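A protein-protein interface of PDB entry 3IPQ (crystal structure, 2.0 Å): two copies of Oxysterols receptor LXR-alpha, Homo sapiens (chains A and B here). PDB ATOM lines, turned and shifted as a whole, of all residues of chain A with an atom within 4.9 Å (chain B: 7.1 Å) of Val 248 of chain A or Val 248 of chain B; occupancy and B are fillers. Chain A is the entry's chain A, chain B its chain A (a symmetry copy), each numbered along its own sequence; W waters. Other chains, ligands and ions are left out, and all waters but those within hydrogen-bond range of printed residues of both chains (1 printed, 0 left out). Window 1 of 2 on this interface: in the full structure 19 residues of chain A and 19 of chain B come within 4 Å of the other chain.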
ATOM      1  N   LEU A 244      32.659   6.733 -11.665  1.00  0.00           N
ATOM      2  CA  LEU A 244      31.722   7.280 -12.661  1.00  0.00           C
ATOM      3  C   LEU A 244      31.676   8.792 -12.659  1.00  0.00           C
ATOM      4  O   LEU A 244      31.594   9.401 -13.731  1.00  0.00           O
ATOM      5  CB  LEU A 244      30.298   6.715 -12.509  1.00  0.00           C
ATOM      6  CG  LEU A 244      30.004   5.256 -12.869  1.00  0.00           C
ATOM      7  CD1 LEU A 244      28.497   5.030 -12.690  1.00  0.00           C
ATOM      8  CD2 LEU A 244      30.476   4.743 -14.278  1.00  0.00           C
ATOM      9  N   MET A 245      31.755   9.400 -11.483  1.00  0.00           N
ATOM     10  CA  MET A 245      31.673  10.856 -11.349  1.00  0.00           C
ATOM     11  C   MET A 245      32.887  11.585 -11.969  1.00  0.00           C
ATOM     12  O   MET A 245      32.822  12.790 -12.294  1.00  0.00           O
ATOM     13  CB  MET A 245      31.467  11.254  -9.862  1.00  0.00           C
ATOM     14  CG  MET A 245      30.056  10.852  -9.215  1.00  0.00           C
ATOM     15  SD  MET A 245      28.700  11.668 -10.028  1.00  0.00           S
ATOM     16  CE  MET A 245      28.891  13.314  -9.361  1.00  0.00           C
ATOM     17  N   LYS A 246      33.986  10.871 -12.168  1.00  0.00           N
ATOM     18  CA  LYS A 246      35.137  11.469 -12.848  1.00  0.00           C
ATOM     19  C   LYS A 246      34.857  11.760 -14.311  1.00  0.00           C
ATOM     20  O   LYS A 246      35.504  12.623 -14.895  1.00  0.00           O
ATOM     21  CB  LYS A 246      36.392  10.589 -12.688  1.00  0.00           C
ATOM     22  CG  LYS A 246      36.931  10.539 -11.258  1.00  0.00           C
ATOM     23  CD  LYS A 246      37.565  11.872 -10.842  1.00  0.00           C
ATOM     24  CE  LYS A 246      37.910  11.941  -9.335  1.00  0.00           C
ATOM     25  NZ  LYS A 246      37.124  12.983  -8.654  1.00  0.00           N
ATOM     26  N   LEU A 247      33.911  11.026 -14.901  1.00  0.00           N
ATOM     27  CA  LEU A 247      33.468  11.265 -16.269  1.00  0.00           C
ATOM     28  C   LEU A 247      32.824  12.636 -16.438  1.00  0.00           C
ATOM     29  O   LEU A 247      32.858  13.227 -17.525  1.00  0.00           O
ATOM     30  CB  LEU A 247      32.495  10.184 -16.721  1.00  0.00           C
ATOM     31  CG  LEU A 247      33.083   8.757 -16.706  1.00  0.00           C
ATOM     32  CD1 LEU A 247      32.024   7.736 -17.049  1.00  0.00           C
ATOM     33  CD2 LEU A 247      34.299   8.632 -17.609  1.00  0.00           C
ATOM     34  N   VAL A 248      32.230  13.116 -15.367  1.00  0.00           N
ATOM     35  CA  VAL A 248      31.656  14.462 -15.306  1.00  0.00           C
ATOM     36  C   VAL A 248      32.770  15.514 -15.411  1.00  0.00           C
ATOM     37  O   VAL A 248      32.671  16.438 -16.202  1.00  0.00           O
ATOM     38  CB  VAL A 248      30.870  14.658 -13.989  1.00  0.00           C
ATOM     39  CG1 VAL A 248      30.246  16.046 -13.922  1.00  0.00           C
ATOM     40  CG2 VAL A 248      29.797  13.584 -13.838  1.00  0.00           C
ATOM     41  N   SER A 249      33.837  15.343 -14.624  1.00  0.00           N
ATOM     42  CA  SER A 249      35.006  16.250 -14.675  1.00  0.00           C
ATOM     43  C   SER A 249      35.644  16.251 -16.043  1.00  0.00           C
ATOM     44  O   SER A 249      36.010  17.303 -16.576  1.00  0.00           O
ATOM     45  CB  SER A 249      36.037  15.823 -13.635  1.00  0.00           C
ATOM     46  OG  SER A 249      35.467  15.917 -12.344  1.00  0.00           O
ATOM     47  N   LEU A 250      35.745  15.071 -16.645  1.00  0.00           N
ATOM     48  CA  LEU A 250      36.267  14.971 -18.007  1.00  0.00           C
ATOM     49  C   LEU A 250      35.481  15.785 -18.996  1.00  0.00           C
ATOM     50  O   LEU A 250      36.072  16.332 -19.929  1.00  0.00           O
ATOM     51  CB  LEU A 250      36.312  13.518 -18.474  1.00  0.00           C
ATOM     52  CG  LEU A 250      37.391  12.659 -17.893  1.00  0.00           C
ATOM     53  CD1 LEU A 250      37.124  11.143 -18.238  1.00  0.00           C
ATOM     54  CD2 LEU A 250      38.739  13.173 -18.403  1.00  0.00           C
ATOM     55  N   ARG A 251      34.157  15.917 -18.825  1.00  0.00           N
ATOM     56  CA  ARG A 251      33.434  16.776 -19.757  1.00  0.00           C
ATOM     57  C   ARG A 251      33.818  18.235 -19.636  1.00  0.00           C
ATOM     58  O   ARG A 251      33.898  18.915 -20.631  1.00  0.00           O
ATOM     59  CB  ARG A 251      31.932  16.739 -19.592  1.00  0.00           C
ATOM     60  CG  ARG A 251      31.289  15.586 -20.073  1.00  0.00           C
ATOM     61  CD  ARG A 251      31.615  15.242 -21.512  1.00  0.00           C
ATOM     62  NE  ARG A 251      31.064  13.931 -21.729  1.00  0.00           N
ATOM     63  CZ  ARG A 251      29.879  13.692 -22.255  1.00  0.00           C
ATOM     64  NH1 ARG A 251      29.102  14.678 -22.641  1.00  0.00           N
ATOM     65  NH2 ARG A 251      29.478  12.440 -22.396  1.00  0.00           N
ATOM     66  N   THR A 252      33.990  18.733 -18.429  1.00  0.00           N
ATOM     67  CA  THR A 252      34.433  20.114 -18.261  1.00  0.00           C
ATOM     68  C   THR A 252      35.829  20.335 -18.846  1.00  0.00           C
ATOM     69  O   THR A 252      36.103  21.366 -19.502  1.00  0.00           O
ATOM     70  CB  THR A 252      34.417  20.507 -16.823  1.00  0.00           C
ATOM     71  OG1 THR A 252      33.063  20.525 -16.385  1.00  0.00           O
ATOM     72  CG2 THR A 252      35.052  21.889 -16.650  1.00  0.00           C
ATOM     73  N   GLU B 132      22.831  24.040 -14.488  1.00  0.00           N
ATOM     74  CA  GLU B 132      22.614  22.574 -14.473  1.00  0.00           C
ATOM     75  C   GLU B 132      21.317  22.244 -13.751  1.00  0.00           C
ATOM     76  O   GLU B 132      20.491  21.460 -14.258  1.00  0.00           O
ATOM     77  CB  GLU B 132      23.816  21.878 -13.818  1.00  0.00           C
ATOM     78  CG  GLU B 132      25.016  22.026 -14.621  1.00  0.00           C
ATOM     79  CD  GLU B 132      26.198  21.235 -14.110  1.00  0.00           C
ATOM     80  OE1 GLU B 132      26.023  20.291 -13.312  1.00  0.00           O
ATOM     81  OE2 GLU B 132      27.302  21.572 -14.509  1.00  0.00           O
ATOM     82  N   PHE B 178      18.090  16.539 -24.326  1.00  0.00           N
ATOM     83  CA  PHE B 178      18.278  16.202 -22.913  1.00  0.00           C
ATOM     84  C   PHE B 178      16.968  15.936 -22.192  1.00  0.00           C
ATOM     85  O   PHE B 178      16.826  14.934 -21.492  1.00  0.00           O
ATOM     86  CB  PHE B 178      19.050  17.339 -22.217  1.00  0.00           C
ATOM     87  CG  PHE B 178      19.275  17.107 -20.763  1.00  0.00           C
ATOM     88  CD1 PHE B 178      20.254  16.209 -20.335  1.00  0.00           C
ATOM     89  CD2 PHE B 178      18.529  17.788 -19.812  1.00  0.00           C
ATOM     90  CE1 PHE B 178      20.447  15.986 -18.960  1.00  0.00           C
ATOM     91  CE2 PHE B 178      18.722  17.570 -18.443  1.00  0.00           C
ATOM     92  CZ  PHE B 178      19.672  16.664 -18.024  1.00  0.00           C
ATOM     93  N   SER B 202      29.389  19.822  -6.146  1.00  0.00           N
ATOM     94  CA  SER B 202      30.452  19.397  -7.041  1.00  0.00           C
ATOM     95  C   SER B 202      31.756  20.099  -6.657  1.00  0.00           C
ATOM     96  O   SER B 202      31.923  21.327  -6.856  1.00  0.00           O
ATOM     97  CB  SER B 202      30.076  19.731  -8.486  1.00  0.00           C
ATOM     98  OG  SER B 202      28.878  19.065  -8.856  1.00  0.00           O
ATOM     99  N   ASP B 204      34.696  20.014  -7.866  1.00  0.00           N
ATOM    100  CA  ASP B 204      35.497  20.478  -8.978  1.00  0.00           C
ATOM    101  C   ASP B 204      35.002  21.807  -9.616  1.00  0.00           C
ATOM    102  O   ASP B 204      35.541  22.225 -10.651  1.00  0.00           O
ATOM    103  CB  ASP B 204      35.602  19.379 -10.049  1.00  0.00           C
ATOM    104  CG  ASP B 204      34.269  19.103 -10.773  1.00  0.00           C
ATOM    105  OD1 ASP B 204      33.158  19.272 -10.194  1.00  0.00           O
ATOM    106  OD2 ASP B 204      34.342  18.672 -11.932  1.00  0.00           O
ATOM    107  N   ARG B 205      34.025  22.491  -9.017  1.00  0.00           N
ATOM    108  CA  ARG B 205      33.592  23.789  -9.586  1.00  0.00           C
ATOM    109  C   ARG B 205      34.750  24.763  -9.433  1.00  0.00           C
ATOM    110  O   ARG B 205      35.527  24.633  -8.457  1.00  0.00           O
ATOM    111  CB  ARG B 205      32.402  24.384  -8.859  1.00  0.00           C
ATOM    112  CG  ARG B 205      31.154  23.593  -8.890  1.00  0.00           C
ATOM    113  CD  ARG B 205      30.702  23.216 -10.273  1.00  0.00           C
ATOM    114  NE  ARG B 205      29.356  22.669 -10.195  1.00  0.00           N
ATOM    115  CZ  ARG B 205      28.696  22.197 -11.234  1.00  0.00           C
ATOM    116  NH1 ARG B 205      29.227  22.235 -12.460  1.00  0.00           N
ATOM    117  NH2 ARG B 205      27.493  21.703 -11.038  1.00  0.00           N
ATOM    118  N   GLN B 218      28.725  15.656  -1.056  1.00  0.00           N
ATOM    119  CA  GLN B 218      28.212  15.058  -2.278  1.00  0.00           C
ATOM    120  C   GLN B 218      28.006  13.542  -2.114  1.00  0.00           C
ATOM    121  O   GLN B 218      27.000  12.996  -2.531  1.00  0.00           O
ATOM    122  CB  GLN B 218      29.163  15.273  -3.465  1.00  0.00           C
ATOM    123  CG  GLN B 218      28.490  14.964  -4.792  1.00  0.00           C
ATOM    124  CD  GLN B 218      29.426  15.052  -5.967  1.00  0.00           C
ATOM    125  OE1 GLN B 218      30.462  14.421  -5.959  1.00  0.00           O
ATOM    126  NE2 GLN B 218      29.006  15.743  -7.043  1.00  0.00           N
ATOM    127  N   MET B 243      21.255   7.509 -13.756  1.00  0.00           N
ATOM    128  CA  MET B 243      20.914   8.816 -13.194  1.00  0.00           C
ATOM    129  C   MET B 243      22.132   9.635 -13.018  1.00  0.00           C
ATOM    130  O   MET B 243      22.190  10.790 -13.480  1.00  0.00           O
ATOM    131  CB  MET B 243      20.227   8.666 -11.824  1.00  0.00           C
ATOM    132  CG  MET B 243      18.854   8.162 -11.975  1.00  0.00           C
ATOM    133  SD  MET B 243      18.059   7.980 -10.367  1.00  0.00           S
ATOM    134  CE  MET B 243      16.697   6.885 -10.847  1.00  0.00           C
ATOM    135  N   LEU B 244      23.141   9.035 -12.389  1.00  0.00           N
ATOM    136  CA  LEU B 244      24.437   9.712 -12.212  1.00  0.00           C
ATOM    137  C   LEU B 244      25.054  10.155 -13.519  1.00  0.00           C
ATOM    138  O   LEU B 244      25.633  11.244 -13.583  1.00  0.00           O
ATOM    139  CB  LEU B 244      25.447   8.863 -11.419  1.00  0.00           C
ATOM    140  CG  LEU B 244      25.242   8.620  -9.921  1.00  0.00           C
ATOM    141  CD1 LEU B 244      26.448   7.818  -9.414  1.00  0.00           C
ATOM    142  CD2 LEU B 244      24.987   9.872  -9.006  1.00  0.00           C
ATOM    143  N   MET B 245      24.916   9.345 -14.560  1.00  0.00           N
ATOM    144  CA  MET B 245      25.511   9.641 -15.865  1.00  0.00           C
ATOM    145  C   MET B 245      24.870  10.868 -16.553  1.00  0.00           C
ATOM    146  O   MET B 245      25.470  11.495 -17.451  1.00  0.00           O
ATOM    147  CB  MET B 245      25.466   8.387 -16.780  1.00  0.00           C
ATOM    148  CG  MET B 245      26.401   7.161 -16.340  1.00  0.00           C
ATOM    149  SD  MET B 245      28.124   7.601 -16.366  1.00  0.00           S
ATOM    150  CE  MET B 245      28.413   7.595 -18.129  1.00  0.00           C
ATOM    151  N   LYS B 246      23.671  11.243 -16.128  1.00  0.00           N
ATOM    152  CA  LYS B 246      23.051  12.459 -16.660  1.00  0.00           C
ATOM    153  C   LYS B 246      23.784  13.717 -16.231  1.00  0.00           C
ATOM    154  O   LYS B 246      23.688  14.737 -16.905  1.00  0.00           O
ATOM    155  CB  LYS B 246      21.559  12.531 -16.278  1.00  0.00           C
ATOM    156  CG  LYS B 246      20.696  11.473 -16.969  1.00  0.00           C
ATOM    157  CD  LYS B 246      20.536  11.760 -18.468  1.00  0.00           C
ATOM    158  CE  LYS B 246      19.871  10.598 -19.245  1.00  0.00           C
ATOM    159  NZ  LYS B 246      20.794  10.022 -20.236  1.00  0.00           N
ATOM    160  N   LEU B 247      24.495  13.646 -15.103  1.00  0.00           N
ATOM    161  CA  LEU B 247      25.328  14.743 -14.628  1.00  0.00           C
ATOM    162  C   LEU B 247      26.467  15.063 -15.589  1.00  0.00           C
ATOM    163  O   LEU B 247      26.940  16.205 -15.660  1.00  0.00           O
ATOM    164  CB  LEU B 247      25.895  14.436 -13.249  1.00  0.00           C
ATOM    165  CG  LEU B 247      24.824  14.211 -12.160  1.00  0.00           C
ATOM    166  CD1 LEU B 247      25.462  13.795 -10.856  1.00  0.00           C
ATOM    167  CD2 LEU B 247      23.926  15.425 -11.985  1.00  0.00           C
ATOM    168  N   VAL B 248      26.905  14.049 -16.303  1.00  0.00           N
ATOM    169  CA  VAL B 248      27.914  14.187 -17.356  1.00  0.00           C
ATOM    170  C   VAL B 248      27.352  15.025 -18.514  1.00  0.00           C
ATOM    171  O   VAL B 248      27.995  15.960 -18.965  1.00  0.00           O
ATOM    172  CB  VAL B 248      28.350  12.798 -17.876  1.00  0.00           C
ATOM    173  CG1 VAL B 248      29.417  12.925 -18.955  1.00  0.00           C
ATOM    174  CG2 VAL B 248      28.854  11.929 -16.728  1.00  0.00           C
ATOM    175  N   SER B 249      26.138  14.695 -18.965  1.00  0.00           N
ATOM    176  CA  SER B 249      25.459  15.463 -20.034  1.00  0.00           C
ATOM    177  C   SER B 249      25.242  16.900 -19.627  1.00  0.00           C
ATOM    178  O   SER B 249      25.455  17.826 -20.415  1.00  0.00           O
ATOM    179  CB  SER B 249      24.115  14.819 -20.358  1.00  0.00           C
ATOM    180  OG  SER B 249      24.328  13.504 -20.834  1.00  0.00           O
ATOM    181  N   LEU B 250      24.855  17.103 -18.372  1.00  0.00           N
ATOM    182  CA  LEU B 250      24.701  18.461 -17.850  1.00  0.00           C
ATOM    183  C   LEU B 250      25.963  19.271 -17.947  1.00  0.00           C
ATOM    184  O   LEU B 250      25.885  20.477 -18.186  1.00  0.00           O
ATOM    185  CB  LEU B 250      24.226  18.441 -16.399  1.00  0.00           C
ATOM    186  CG  LEU B 250      22.791  18.084 -16.168  1.00  0.00           C
ATOM    187  CD1 LEU B 250      22.537  17.820 -14.633  1.00  0.00           C
ATOM    188  CD2 LEU B 250      21.920  19.201 -16.747  1.00  0.00           C
ATOM    189  N   ARG B 251      27.145  18.656 -17.796  1.00  0.00           N
ATOM    190  CA  ARG B 251      28.354  19.455 -17.971  1.00  0.00           C
ATOM    191  C   ARG B 251      28.539  19.943 -19.393  1.00  0.00           C
ATOM    192  O   ARG B 251      28.982  21.048 -19.592  1.00  0.00           O
ATOM    193  CB  ARG B 251      29.632  18.726 -17.625  1.00  0.00           C
ATOM    194  CG  ARG B 251      29.885  18.548 -16.254  1.00  0.00           C
ATOM    195  CD  ARG B 251      29.832  19.823 -15.438  1.00  0.00           C
ATOM    196  NE  ARG B 251      29.875  19.402 -14.062  1.00  0.00           N
ATOM    197  CZ  ARG B 251      30.971  19.335 -13.332  1.00  0.00           C
ATOM    198  NH1 ARG B 251      32.136  19.676 -13.833  1.00  0.00           N
ATOM    199  NH2 ARG B 251      30.885  18.923 -12.079  1.00  0.00           N
ATOM    200  N   THR B 252      28.269  19.107 -20.374  1.00  0.00           N
ATOM    201  CA  THR B 252      28.360  19.552 -21.762  1.00  0.00           C
ATOM    202  C   THR B 252      27.353  20.663 -22.067  1.00  0.00           C
ATOM    203  O   THR B 252      27.671  21.654 -22.763  1.00  0.00           O
ATOM    204  CB  THR B 252      28.157  18.411 -22.701  1.00  0.00           C
ATOM    205  OG1 THR B 252      29.255  17.518 -22.554  1.00  0.00           O
ATOM    206  CG2 THR B 252      28.077  18.924 -24.141  1.00  0.00           C
ATOM    207  N   LEU B 253      26.156  20.516 -21.512  1.00  0.00           N
ATOM    208  CA  LEU B 253      25.098  21.500 -21.693  1.00  0.00           C
ATOM    209  C   LEU B 253      25.420  22.853 -21.079  1.00  0.00           C
ATOM    210  O   LEU B 253      24.961  23.903 -21.589  1.00  0.00           O
ATOM    211  CB  LEU B 253      23.779  20.992 -21.124  1.00  0.00           C
ATOM    212  CG  LEU B 253      22.989  20.004 -21.976  1.00  0.00           C
ATOM    213  CD1 LEU B 253      21.856  19.383 -21.151  1.00  0.00           C
ATOM    214  CD2 LEU B 253      22.450  20.674 -23.285  1.00  0.00           C
HETATM  215  O   HOH W   1      36.181  19.483 -14.112  1.00  0.00           O
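OG of Ser 249 of chain A lies within hydrogen-bond range of OD2 of Asp 204 of chain B (3.0 Å). The guanidinium group (NH1) of Arg 251 of chain A sits at hydrogen-bond distance from the side-chain hydroxyl (OG1) of Thr 252 of chain B. The side-chain hydroxyl (OG1) of Thr 252 of chain A is in hydrogen-bond range of the guanidinium group (NH1) of Arg 251 of chain B (2.8 Å).
OE2 of Glu 132 of chain B is in salt-bridge range of NE of Arg 251 of chain B (3.4 Å). The guanidinium group (NH2) of Arg 251 of chain B lies within salt-bridge range of the side-chain carboxylate (OD1) of Asp 204 of chain B (3.0 Å).
Among the printed residues, pairs that only touch across the chains: Met 245 of chain A with Gln 218 of chain B (3.4 Å), Arg 251 of chain A with Val 248 of chain B (3.4 Å), Val 248 of chain A with Arg 251 of chain B (3.4 Å), Val 248 of chain A with Val 248 of chain B (3.5 Å), Arg 251 of chain A with Arg 251 of chain B (3.6 Å), Val 248 of chain A with Leu 247 of chain B (3.7 Å), Leu 247 of chain A with Val 248 of chain B (3.7 Å), Met 245 of chain A with Leu 247 of chain B (3.8 Å) and Leu 247 of chain A with Met 245 of chain B (3.8 Å).
Of chain B, only Leu 247 (3.7 Å), Val 248 (3.5 Å) and Arg 251 (3.4 Å) come within 4 Å of Val 248 of chain A. Val 248 of chain B touches just these residues of chain A: Leu 247, Val 248 and Arg 251. Of the printed residues of chain A, Met 245 of chain B touches Leu 247. Printed residues of chain A within 4 Å of Leu 247 of chain B: Met 245 (3.8 Å) and Val 248 (3.7 Å). Lys 246 of chain B touches none of the printed residues of chain A. Glu 132 of chain B touches none of the printed residues of chain A. The nearest residue of chain A that does not touch Val 248 of chain B is Leu 244 of chain A (4.8 Å).
Hydrophobic or aromatic side chains of chain B within 4 Å of the printed part of chain A: Met 245, Leu 247 and Val 248. Of the 9 printed residues of chain A, 6 touch a printed residue of chain B. Printed residues of chain A that touch a printed residue of chain B: Met 245, Leu 247, Val 248, Ser 249, Arg 251 and Thr 252. Hydrophobic or aromatic side chains of chain A within 4 Å of the printed part of chain B: Met 245, Leu 247 and Val 248. Among the printed residues, 12 pairs touch across the chains. Among the printed residues, no Asp or Glu carboxylate lies within 4 Å of a Lys or Arg side-chain nitrogen of the other chain.
Leu 247 of chain A touches Val 248 of chain B, and with the chains exchanged Val 248 of chain A touches Leu 247 of chain B. Val 248 of chain B touches its own counterpart, Val 248 of chain A. Val 248 of chain A touches Arg 251 of chain B, and with the chains exchanged Arg 251 of chain A touches Val 248 of chain B. Arg 251 of chain A touches its own counterpart, Arg 251 of chain B. Positions printed for both chains: 244, 245, 246, 247, 248, 249, 250, 251 and 252.
Water W1 bridges the side-chain carboxylate (OD2) of Asp 204 of chain B (3.0 Å) and the backbone carbonyl oxygen (O) of Ser 249 of chain A (3.3 Å).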
